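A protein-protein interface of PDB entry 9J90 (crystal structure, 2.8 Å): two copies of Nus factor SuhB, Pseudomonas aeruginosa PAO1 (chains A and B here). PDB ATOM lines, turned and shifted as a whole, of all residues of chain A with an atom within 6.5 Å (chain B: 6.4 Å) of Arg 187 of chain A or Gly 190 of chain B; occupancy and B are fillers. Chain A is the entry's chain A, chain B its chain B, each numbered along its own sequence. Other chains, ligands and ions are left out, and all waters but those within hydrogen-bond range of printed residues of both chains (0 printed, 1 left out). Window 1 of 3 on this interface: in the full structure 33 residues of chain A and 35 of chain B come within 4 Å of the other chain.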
ATOM      1  N   LEU A 154      11.541  -1.963 -26.139  1.00  0.00           N
ATOM      2  CA  LEU A 154      12.510  -2.969 -25.650  1.00  0.00           C
ATOM      3  C   LEU A 154      12.993  -2.511 -24.292  1.00  0.00           C
ATOM      4  O   LEU A 154      13.673  -1.460 -24.206  1.00  0.00           O
ATOM      5  CB  LEU A 154      13.685  -3.103 -26.633  1.00  0.00           C
ATOM      6  CG  LEU A 154      14.754  -4.120 -26.226  1.00  0.00           C
ATOM      7  CD1 LEU A 154      14.170  -5.541 -26.124  1.00  0.00           C
ATOM      8  CD2 LEU A 154      15.926  -4.041 -27.183  1.00  0.00           C
ATOM      9  N   LEU A 155      12.664  -3.274 -23.278  1.00  0.00           N
ATOM     10  CA  LEU A 155      12.998  -2.890 -21.890  1.00  0.00           C
ATOM     11  C   LEU A 155      14.164  -3.718 -21.395  1.00  0.00           C
ATOM     12  O   LEU A 155      14.305  -4.885 -21.723  1.00  0.00           O
ATOM     13  CB  LEU A 155      11.771  -3.089 -20.998  1.00  0.00           C
ATOM     14  CG  LEU A 155      10.520  -2.388 -21.496  1.00  0.00           C
ATOM     15  CD1 LEU A 155       9.371  -2.645 -20.546  1.00  0.00           C
ATOM     16  CD2 LEU A 155      10.789  -0.898 -21.643  1.00  0.00           C
ATOM     17  N   GLY A 156      14.830  -3.168 -20.396  1.00  0.00           N
ATOM     18  CA  GLY A 156      15.836  -3.910 -19.627  1.00  0.00           C
ATOM     19  C   GLY A 156      15.346  -4.213 -18.236  1.00  0.00           C
ATOM     20  O   GLY A 156      14.525  -3.479 -17.714  1.00  0.00           O
ATOM     21  N   THR A 157      15.837  -5.271 -17.635  1.00  0.00           N
ATOM     22  CA  THR A 157      15.465  -5.576 -16.254  1.00  0.00           C
ATOM     23  C   THR A 157      16.428  -6.560 -15.636  1.00  0.00           C
ATOM     24  O   THR A 157      17.362  -7.041 -16.303  1.00  0.00           O
ATOM     25  CB  THR A 157      13.984  -5.968 -16.115  1.00  0.00           C
ATOM     26  OG1 THR A 157      13.643  -5.883 -14.724  1.00  0.00           O
ATOM     27  CG2 THR A 157      13.681  -7.344 -16.666  1.00  0.00           C
ATOM     28  N   GLY A 158      16.192  -6.911 -14.406  1.00  0.00           N
ATOM     29  CA  GLY A 158      17.069  -7.797 -13.628  1.00  0.00           C
ATOM     30  C   GLY A 158      16.515  -8.094 -12.254  1.00  0.00           C
ATOM     31  O   GLY A 158      15.764  -7.291 -11.680  1.00  0.00           O
ATOM     32  N   ALA A 184       7.888  -5.075 -27.146  1.00  0.00           N
ATOM     33  CA  ALA A 184       8.455  -6.009 -28.130  1.00  0.00           C
ATOM     34  C   ALA A 184       9.363  -7.017 -27.430  1.00  0.00           C
ATOM     35  O   ALA A 184       9.578  -8.137 -27.942  1.00  0.00           O
ATOM     36  CB  ALA A 184       9.217  -5.226 -29.178  1.00  0.00           C
ATOM     37  N   GLY A 185       9.931  -6.644 -26.302  1.00  0.00           N
ATOM     38  CA  GLY A 185      10.778  -7.565 -25.553  1.00  0.00           C
ATOM     39  C   GLY A 185      11.183  -6.975 -24.230  1.00  0.00           C
ATOM     40  O   GLY A 185      11.231  -5.748 -24.065  1.00  0.00           O
ATOM     41  N   ILE A 186      11.503  -7.875 -23.314  1.00  0.00           N
ATOM     42  CA  ILE A 186      12.253  -7.578 -22.078  1.00  0.00           C
ATOM     43  C   ILE A 186      13.561  -8.363 -22.146  1.00  0.00           C
ATOM     44  O   ILE A 186      13.548  -9.539 -22.472  1.00  0.00           O
ATOM     45  CB  ILE A 186      11.378  -7.914 -20.865  1.00  0.00           C
ATOM     46  CG1 ILE A 186      10.022  -7.239 -21.031  1.00  0.00           C
ATOM     47  CG2 ILE A 186      12.092  -7.507 -19.585  1.00  0.00           C
ATOM     48  CD1 ILE A 186       9.011  -7.675 -20.041  1.00  0.00           C
ATOM     49  N   ARG A 187      14.656  -7.704 -21.797  1.00  0.00           N
ATOM     50  CA  ARG A 187      15.988  -8.300 -21.768  1.00  0.00           C
ATOM     51  C   ARG A 187      16.543  -8.335 -20.354  1.00  0.00           C
ATOM     52  O   ARG A 187      16.468  -7.304 -19.673  1.00  0.00           O
ATOM     53  CB  ARG A 187      16.964  -7.511 -22.631  1.00  0.00           C
ATOM     54  CG  ARG A 187      16.594  -7.465 -24.101  1.00  0.00           C
ATOM     55  CD  ARG A 187      17.098  -8.665 -24.888  1.00  0.00           C
ATOM     56  NE  ARG A 187      16.559  -8.739 -26.241  1.00  0.00           N
ATOM     57  CZ  ARG A 187      15.342  -9.146 -26.552  1.00  0.00           C
ATOM     58  NH1 ARG A 187      14.473  -9.467 -25.596  1.00  0.00           N
ATOM     59  NH2 ARG A 187      14.984  -9.152 -27.825  1.00  0.00           N
ATOM     60  N   ARG A 188      17.166  -9.451 -20.018  1.00  0.00           N
ATOM     61  CA  ARG A 188      17.849  -9.668 -18.736  1.00  0.00           C
ATOM     62  C   ARG A 188      19.302 -10.055 -19.013  1.00  0.00           C
ATOM     63  O   ARG A 188      19.587 -11.219 -19.127  1.00  0.00           O
ATOM     64  CB  ARG A 188      17.063 -10.737 -17.989  1.00  0.00           C
ATOM     65  CG  ARG A 188      17.216 -10.710 -16.481  1.00  0.00           C
ATOM     66  CD  ARG A 188      16.661 -12.010 -15.902  1.00  0.00           C
ATOM     67  NE  ARG A 188      15.253 -12.249 -16.218  1.00  0.00           N
ATOM     68  CZ  ARG A 188      14.232 -11.626 -15.625  1.00  0.00           C
ATOM     69  NH1 ARG A 188      14.468 -10.732 -14.669  1.00  0.00           N
ATOM     70  NH2 ARG A 188      12.987 -11.892 -16.009  1.00  0.00           N
ATOM     71  N   ALA A 189      20.163  -9.064 -19.146  1.00  0.00           N
ATOM     72  CA  ALA A 189      21.519  -9.193 -19.683  1.00  0.00           C
ATOM     73  C   ALA A 189      22.542  -9.449 -18.594  1.00  0.00           C
ATOM     74  O   ALA A 189      23.624 -10.040 -18.904  1.00  0.00           O
ATOM     75  CB  ALA A 189      21.826  -7.919 -20.427  1.00  0.00           C
ATOM     76  N   GLY A 190      22.265  -8.939 -17.381  1.00  0.00           N
ATOM     77  CA  GLY A 190      23.049  -9.282 -16.173  1.00  0.00           C
ATOM     78  C   GLY A 190      24.092  -8.276 -15.748  1.00  0.00           C
ATOM     79  O   GLY A 190      24.998  -8.646 -14.994  1.00  0.00           O
ATOM     80  N   ASP A 195      22.905  -1.890 -18.449  1.00  0.00           N
ATOM     81  CA  ASP A 195      21.483  -1.662 -18.784  1.00  0.00           C
ATOM     82  C   ASP A 195      21.172  -0.175 -18.749  1.00  0.00           C
ATOM     83  O   ASP A 195      20.488   0.332 -19.634  1.00  0.00           O
ATOM     84  CB  ASP A 195      20.552  -2.544 -17.950  1.00  0.00           C
ATOM     85  CG  ASP A 195      20.764  -4.030 -18.142  1.00  0.00           C
ATOM     86  OD1 ASP A 195      21.514  -4.436 -19.115  1.00  0.00           O
ATOM     87  OD2 ASP A 195      20.202  -4.764 -17.334  1.00  0.00           O
ATOM     88  N   TYR A 204      17.964   0.560 -25.028  1.00  0.00           N
ATOM     89  CA  TYR A 204      16.718   0.213 -24.330  1.00  0.00           C
ATOM     90  C   TYR A 204      15.854   1.443 -24.201  1.00  0.00           C
ATOM     91  O   TYR A 204      16.401   2.542 -24.019  1.00  0.00           O
ATOM     92  CB  TYR A 204      17.023  -0.333 -22.934  1.00  0.00           C
ATOM     93  CG  TYR A 204      17.757  -1.648 -22.868  1.00  0.00           C
ATOM     94  CD1 TYR A 204      17.732  -2.558 -23.901  1.00  0.00           C
ATOM     95  CD2 TYR A 204      18.419  -2.010 -21.714  1.00  0.00           C
ATOM     96  CE1 TYR A 204      18.400  -3.773 -23.804  1.00  0.00           C
ATOM     97  CE2 TYR A 204      19.086  -3.216 -21.590  1.00  0.00           C
ATOM     98  CZ  TYR A 204      19.066  -4.108 -22.637  1.00  0.00           C
ATOM     99  OH  TYR A 204      19.685  -5.309 -22.502  1.00  0.00           O
ATOM    100  N   PHE A 207      14.067   0.758 -18.321  1.00  0.00           N
ATOM    101  CA  PHE A 207      14.733  -0.245 -17.457  1.00  0.00           C
ATOM    102  C   PHE A 207      14.161  -0.083 -16.064  1.00  0.00           C
ATOM    103  O   PHE A 207      13.937   1.039 -15.629  1.00  0.00           O
ATOM    104  CB  PHE A 207      16.241   0.030 -17.460  1.00  0.00           C
ATOM    105  CG  PHE A 207      17.010  -0.653 -16.370  1.00  0.00           C
ATOM    106  CD1 PHE A 207      17.415  -1.964 -16.527  1.00  0.00           C
ATOM    107  CD2 PHE A 207      17.304   0.005 -15.203  1.00  0.00           C
ATOM    108  CE1 PHE A 207      18.107  -2.624 -15.525  1.00  0.00           C
ATOM    109  CE2 PHE A 207      18.013  -0.638 -14.207  1.00  0.00           C
ATOM    110  CZ  PHE A 207      18.412  -1.950 -14.368  1.00  0.00           C
ATOM    111  N   ASP B  89      19.526 -13.309 -36.873  1.00  0.00           N
ATOM    112  CA  ASP B  89      18.828 -13.792 -35.665  1.00  0.00           C
ATOM    113  C   ASP B  89      19.014 -12.778 -34.552  1.00  0.00           C
ATOM    114  O   ASP B  89      20.147 -12.466 -34.164  1.00  0.00           O
ATOM    115  CB  ASP B  89      19.260 -15.198 -35.228  1.00  0.00           C
ATOM    116  CG  ASP B  89      18.459 -15.724 -34.054  1.00  0.00           C
ATOM    117  OD1 ASP B  89      17.264 -15.481 -34.010  1.00  0.00           O
ATOM    118  OD2 ASP B  89      19.044 -16.361 -33.180  1.00  0.00           O
ATOM    119  N   GLY B  90      17.891 -12.272 -34.060  1.00  0.00           N
ATOM    120  CA  GLY B  90      17.841 -11.253 -32.985  1.00  0.00           C
ATOM    121  C   GLY B  90      17.541  -9.881 -33.585  1.00  0.00           C
ATOM    122  O   GLY B  90      18.282  -8.886 -33.382  1.00  0.00           O
ATOM    123  N   THR B  91      16.437  -9.826 -34.331  1.00  0.00           N
ATOM    124  CA  THR B  91      16.004  -8.616 -35.059  1.00  0.00           C
ATOM    125  C   THR B  91      15.538  -7.497 -34.127  1.00  0.00           C
ATOM    126  O   THR B  91      15.728  -6.331 -34.478  1.00  0.00           O
ATOM    127  CB  THR B  91      14.922  -8.934 -36.112  1.00  0.00           C
ATOM    128  OG1 THR B  91      13.869  -9.604 -35.450  1.00  0.00           O
ATOM    129  CG2 THR B  91      15.332  -9.849 -37.252  1.00  0.00           C
ATOM    130  N   THR B  92      14.901  -7.818 -33.006  1.00  0.00           N
ATOM    131  CA  THR B  92      14.460  -6.756 -32.084  1.00  0.00           C
ATOM    132  C   THR B  92      15.669  -6.053 -31.478  1.00  0.00           C
ATOM    133  O   THR B  92      15.710  -4.805 -31.453  1.00  0.00           O
ATOM    134  CB  THR B  92      13.563  -7.272 -30.957  1.00  0.00           C
ATOM    135  OG1 THR B  92      12.359  -7.635 -31.614  1.00  0.00           O
ATOM    136  CG2 THR B  92      13.215  -6.247 -29.909  1.00  0.00           C
ATOM    137  N   ASN B  93      16.630  -6.830 -30.998  1.00  0.00           N
ATOM    138  CA  ASN B  93      17.932  -6.269 -30.593  1.00  0.00           C
ATOM    139  C   ASN B  93      18.514  -5.417 -31.713  1.00  0.00           C
ATOM    140  O   ASN B  93      18.858  -4.241 -31.493  1.00  0.00           O
ATOM    141  CB  ASN B  93      18.963  -7.352 -30.286  1.00  0.00           C
ATOM    142  CG  ASN B  93      18.616  -8.086 -29.027  1.00  0.00           C
ATOM    143  OD1 ASN B  93      17.718  -7.654 -28.308  1.00  0.00           O
ATOM    144  ND2 ASN B  93      19.295  -9.188 -28.779  1.00  0.00           N
ATOM    145  N   VAL B  98      20.923  -2.920 -30.062  1.00  0.00           N
ATOM    146  CA  VAL B  98      21.540  -3.791 -29.049  1.00  0.00           C
ATOM    147  C   VAL B  98      22.509  -4.727 -29.771  1.00  0.00           C
ATOM    148  O   VAL B  98      22.103  -5.530 -30.628  1.00  0.00           O
ATOM    149  CB  VAL B  98      20.459  -4.541 -28.269  1.00  0.00           C
ATOM    150  CG1 VAL B  98      21.079  -5.656 -27.427  1.00  0.00           C
ATOM    151  CG2 VAL B  98      19.602  -3.593 -27.439  1.00  0.00           C
ATOM    152  N   HIS B 100      23.738  -7.597 -29.818  1.00  0.00           N
ATOM    153  CA  HIS B 100      23.667  -9.049 -29.573  1.00  0.00           C
ATOM    154  C   HIS B 100      22.705  -9.684 -30.569  1.00  0.00           C
ATOM    155  O   HIS B 100      21.494  -9.655 -30.376  1.00  0.00           O
ATOM    156  CB  HIS B 100      23.235  -9.337 -28.149  1.00  0.00           C
ATOM    157  CG  HIS B 100      23.239 -10.786 -27.756  1.00  0.00           C
ATOM    158  ND1 HIS B 100      24.364 -11.411 -27.257  1.00  0.00           N
ATOM    159  CD2 HIS B 100      22.246 -11.692 -27.701  1.00  0.00           C
ATOM    160  CE1 HIS B 100      24.039 -12.639 -26.918  1.00  0.00           C
ATOM    161  NE2 HIS B 100      22.754 -12.839 -27.194  1.00  0.00           N
ATOM    162  N   PHE B 101      23.276 -10.230 -31.614  1.00  0.00           N
ATOM    163  CA  PHE B 101      22.570 -10.871 -32.740  1.00  0.00           C
ATOM    164  C   PHE B 101      23.611 -11.597 -33.557  1.00  0.00           C
ATOM    165  O   PHE B 101      24.837 -11.295 -33.446  1.00  0.00           O
ATOM    166  CB  PHE B 101      21.833  -9.841 -33.590  1.00  0.00           C
ATOM    167  CG  PHE B 101      22.672  -8.660 -33.993  1.00  0.00           C
ATOM    168  CD1 PHE B 101      23.531  -8.746 -35.074  1.00  0.00           C
ATOM    169  CD2 PHE B 101      22.604  -7.468 -33.286  1.00  0.00           C
ATOM    170  CE1 PHE B 101      24.326  -7.663 -35.433  1.00  0.00           C
ATOM    171  CE2 PHE B 101      23.389  -6.394 -33.653  1.00  0.00           C
ATOM    172  CZ  PHE B 101      24.250  -6.491 -34.719  1.00  0.00           C
ATOM    173  N   THR B 157      17.446 -18.252 -21.750  1.00  0.00           N
ATOM    174  CA  THR B 157      16.071 -18.529 -22.150  1.00  0.00           C
ATOM    175  C   THR B 157      15.493 -17.409 -22.997  1.00  0.00           C
ATOM    176  O   THR B 157      16.177 -16.395 -23.242  1.00  0.00           O
ATOM    177  CB  THR B 157      15.194 -18.893 -20.939  1.00  0.00           C
ATOM    178  OG1 THR B 157      13.999 -19.530 -21.393  1.00  0.00           O
ATOM    179  CG2 THR B 157      14.812 -17.713 -20.082  1.00  0.00           C
ATOM    180  N   ARG B 188      18.059 -13.465 -20.504  1.00  0.00           N
ATOM    181  CA  ARG B 188      17.288 -13.286 -21.754  1.00  0.00           C
ATOM    182  C   ARG B 188      17.996 -12.246 -22.613  1.00  0.00           C
ATOM    183  O   ARG B 188      17.706 -11.092 -22.494  1.00  0.00           O
ATOM    184  CB  ARG B 188      15.867 -12.762 -21.561  1.00  0.00           C
ATOM    185  CG  ARG B 188      14.836 -13.781 -21.115  1.00  0.00           C
ATOM    186  CD  ARG B 188      13.657 -13.066 -20.446  1.00  0.00           C
ATOM    187  NE  ARG B 188      12.981 -12.217 -21.422  1.00  0.00           N
ATOM    188  CZ  ARG B 188      12.046 -12.644 -22.262  1.00  0.00           C
ATOM    189  NH1 ARG B 188      11.632 -13.897 -22.193  1.00  0.00           N
ATOM    190  NH2 ARG B 188      11.492 -11.819 -23.134  1.00  0.00           N
ATOM    191  N   ALA B 189      18.890 -12.701 -23.462  1.00  0.00           N
ATOM    192  CA  ALA B 189      19.732 -11.856 -24.321  1.00  0.00           C
ATOM    193  C   ALA B 189      19.086 -11.525 -25.663  1.00  0.00           C
ATOM    194  O   ALA B 189      19.419 -10.472 -26.242  1.00  0.00           O
ATOM    195  CB  ALA B 189      21.066 -12.555 -24.497  1.00  0.00           C
ATOM    196  N   GLY B 190      18.242 -12.424 -26.163  1.00  0.00           N
ATOM    197  CA  GLY B 190      17.365 -12.168 -27.321  1.00  0.00           C
ATOM    198  C   GLY B 190      17.825 -12.685 -28.670  1.00  0.00           C
ATOM    199  O   GLY B 190      17.362 -12.178 -29.695  1.00  0.00           O
ATOM    200  N   ALA B 191      18.623 -13.728 -28.733  1.00  0.00           N
ATOM    201  CA  ALA B 191      18.973 -14.388 -30.001  1.00  0.00           C
ATOM    202  C   ALA B 191      19.315 -15.826 -29.705  1.00  0.00           C
ATOM    203  O   ALA B 191      20.370 -16.094 -29.089  1.00  0.00           O
ATOM    204  CB  ALA B 191      20.130 -13.683 -30.657  1.00  0.00           C
ATOM    205  N   ALA B 192      18.424 -16.740 -30.102  1.00  0.00           N
ATOM    206  CA  ALA B 192      18.506 -18.158 -29.692  1.00  0.00           C
ATOM    207  C   ALA B 192      19.752 -18.803 -30.261  1.00  0.00           C
ATOM    208  O   ALA B 192      20.329 -19.678 -29.591  1.00  0.00           O
ATOM    209  CB  ALA B 192      17.278 -18.921 -30.122  1.00  0.00           C
ATOM    210  N   ASP B 195      22.391 -17.969 -27.933  1.00  0.00           N
ATOM    211  CA  ASP B 195      22.214 -18.693 -26.653  1.00  0.00           C
ATOM    212  C   ASP B 195      22.721 -20.132 -26.787  1.00  0.00           C
ATOM    213  O   ASP B 195      23.389 -20.637 -25.898  1.00  0.00           O
ATOM    214  CB  ASP B 195      20.792 -18.503 -26.127  1.00  0.00           C
ATOM    215  CG  ASP B 195      20.392 -17.049 -25.846  1.00  0.00           C
ATOM    216  OD1 ASP B 195      21.272 -16.109 -25.844  1.00  0.00           O
ATOM    217  OD2 ASP B 195      19.189 -16.857 -25.667  1.00  0.00           O
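NE of Arg 187 of chain A is in hydrogen-bond range of OD1 of Asn 93 of chain B, 2.6 Å away. The guanidinium group (NE) of Arg 188 of chain B is in hydrogen-bond range of the backbone carbonyl oxygen (O) of Ile 186 of chain A. The backbone NH (N) of Arg 188 of chain A sits at hydrogen-bond distance from the backbone carbonyl oxygen (O) of Arg 188 of chain B. The backbone carbonyl oxygen (O) of Ala 189 of chain B sits close to the guanidinium group (NE) of Arg 187 of chain A (3.3 Å).
CD1 of Leu 154 of chain A touches CG2 of Thr 92 of chain B (3.97 Å). CG2 of Val 98 of chain B touches CD2 of Leu 154 of chain A (3.7 Å). Arg 187 of chain A touches Thr 92 of chain B (NH2 to CB, 3.9 Å). Arg 187 of chain A touches Arg 188 of chain B. Arg 187 of chain A touches Gly 190 of chain B (NE to CA, 3.7 Å). Tyr 204 of chain A touches Val 98 of chain B.
N of Val 98 of chain B is in hydrogen-bond range of O of Asn 93 of chain B (2.8 Å). The side-chain amide nitrogen of Asn 93 of chain B sits at hydrogen-bond distance from the backbone carbonyl oxygen of His 100 of chain B (2.8 Å). ND2 of Asn 93 of chain B sits at hydrogen-bond distance from O of Ala 189 of chain B. O of Leu 155 of chain A sits at hydrogen-bond distance from N of Arg 187 of chain A (2.8 Å). The backbone carbonyl oxygen (O) of Arg 187 of chain A lies within hydrogen-bond range of the backbone NH (N) of Thr 157 of chain A, at 2.9 Å.
Arg 188 of chain A touches its own counterpart, Arg 188 of chain B. Positions printed for both chains: 157, 188, 189, 190 and 195. Of the 10 pairs that touch across the chains among the printed residues, 1 has its exchanged pair printed and touching as well.
Along chain A the printed residues that touch a printed residue of chain B span positions 154 to 204. Hydrophobic or aromatic side chains of chain B that line the printed part of chain A: Val 98. Among the printed residues, 10 pairs touch across the chains.
Of the printed residues of chain B, Leu 154 of chain A touches Thr 92 and Val 98. Printed residues of chain B within 4 Å of Ile 186 of chain A: Arg 188 (2.9 Å). Arg 187 of chain A touches just these residues of chain B: Thr 92 (3.9 Å), Asn 93 (2.6 Å), Arg 188 (3.4 Å), Ala 189 (3.2 Å) and Gly 190 (3.7 Å). Printed residues of chain B within 4 Å of Tyr 204 of chain A: Val 98 (3.8 Å). Thr 157 of chain B touches none of the printed residues of chain A. Gly 190 of chain B touches just one residue of chain A: Arg 187 (3.7 Å). The nearest printed residue of chain A that does not touch Gly 190 of chain B is Ile 186 of chain A (6.6 Å).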
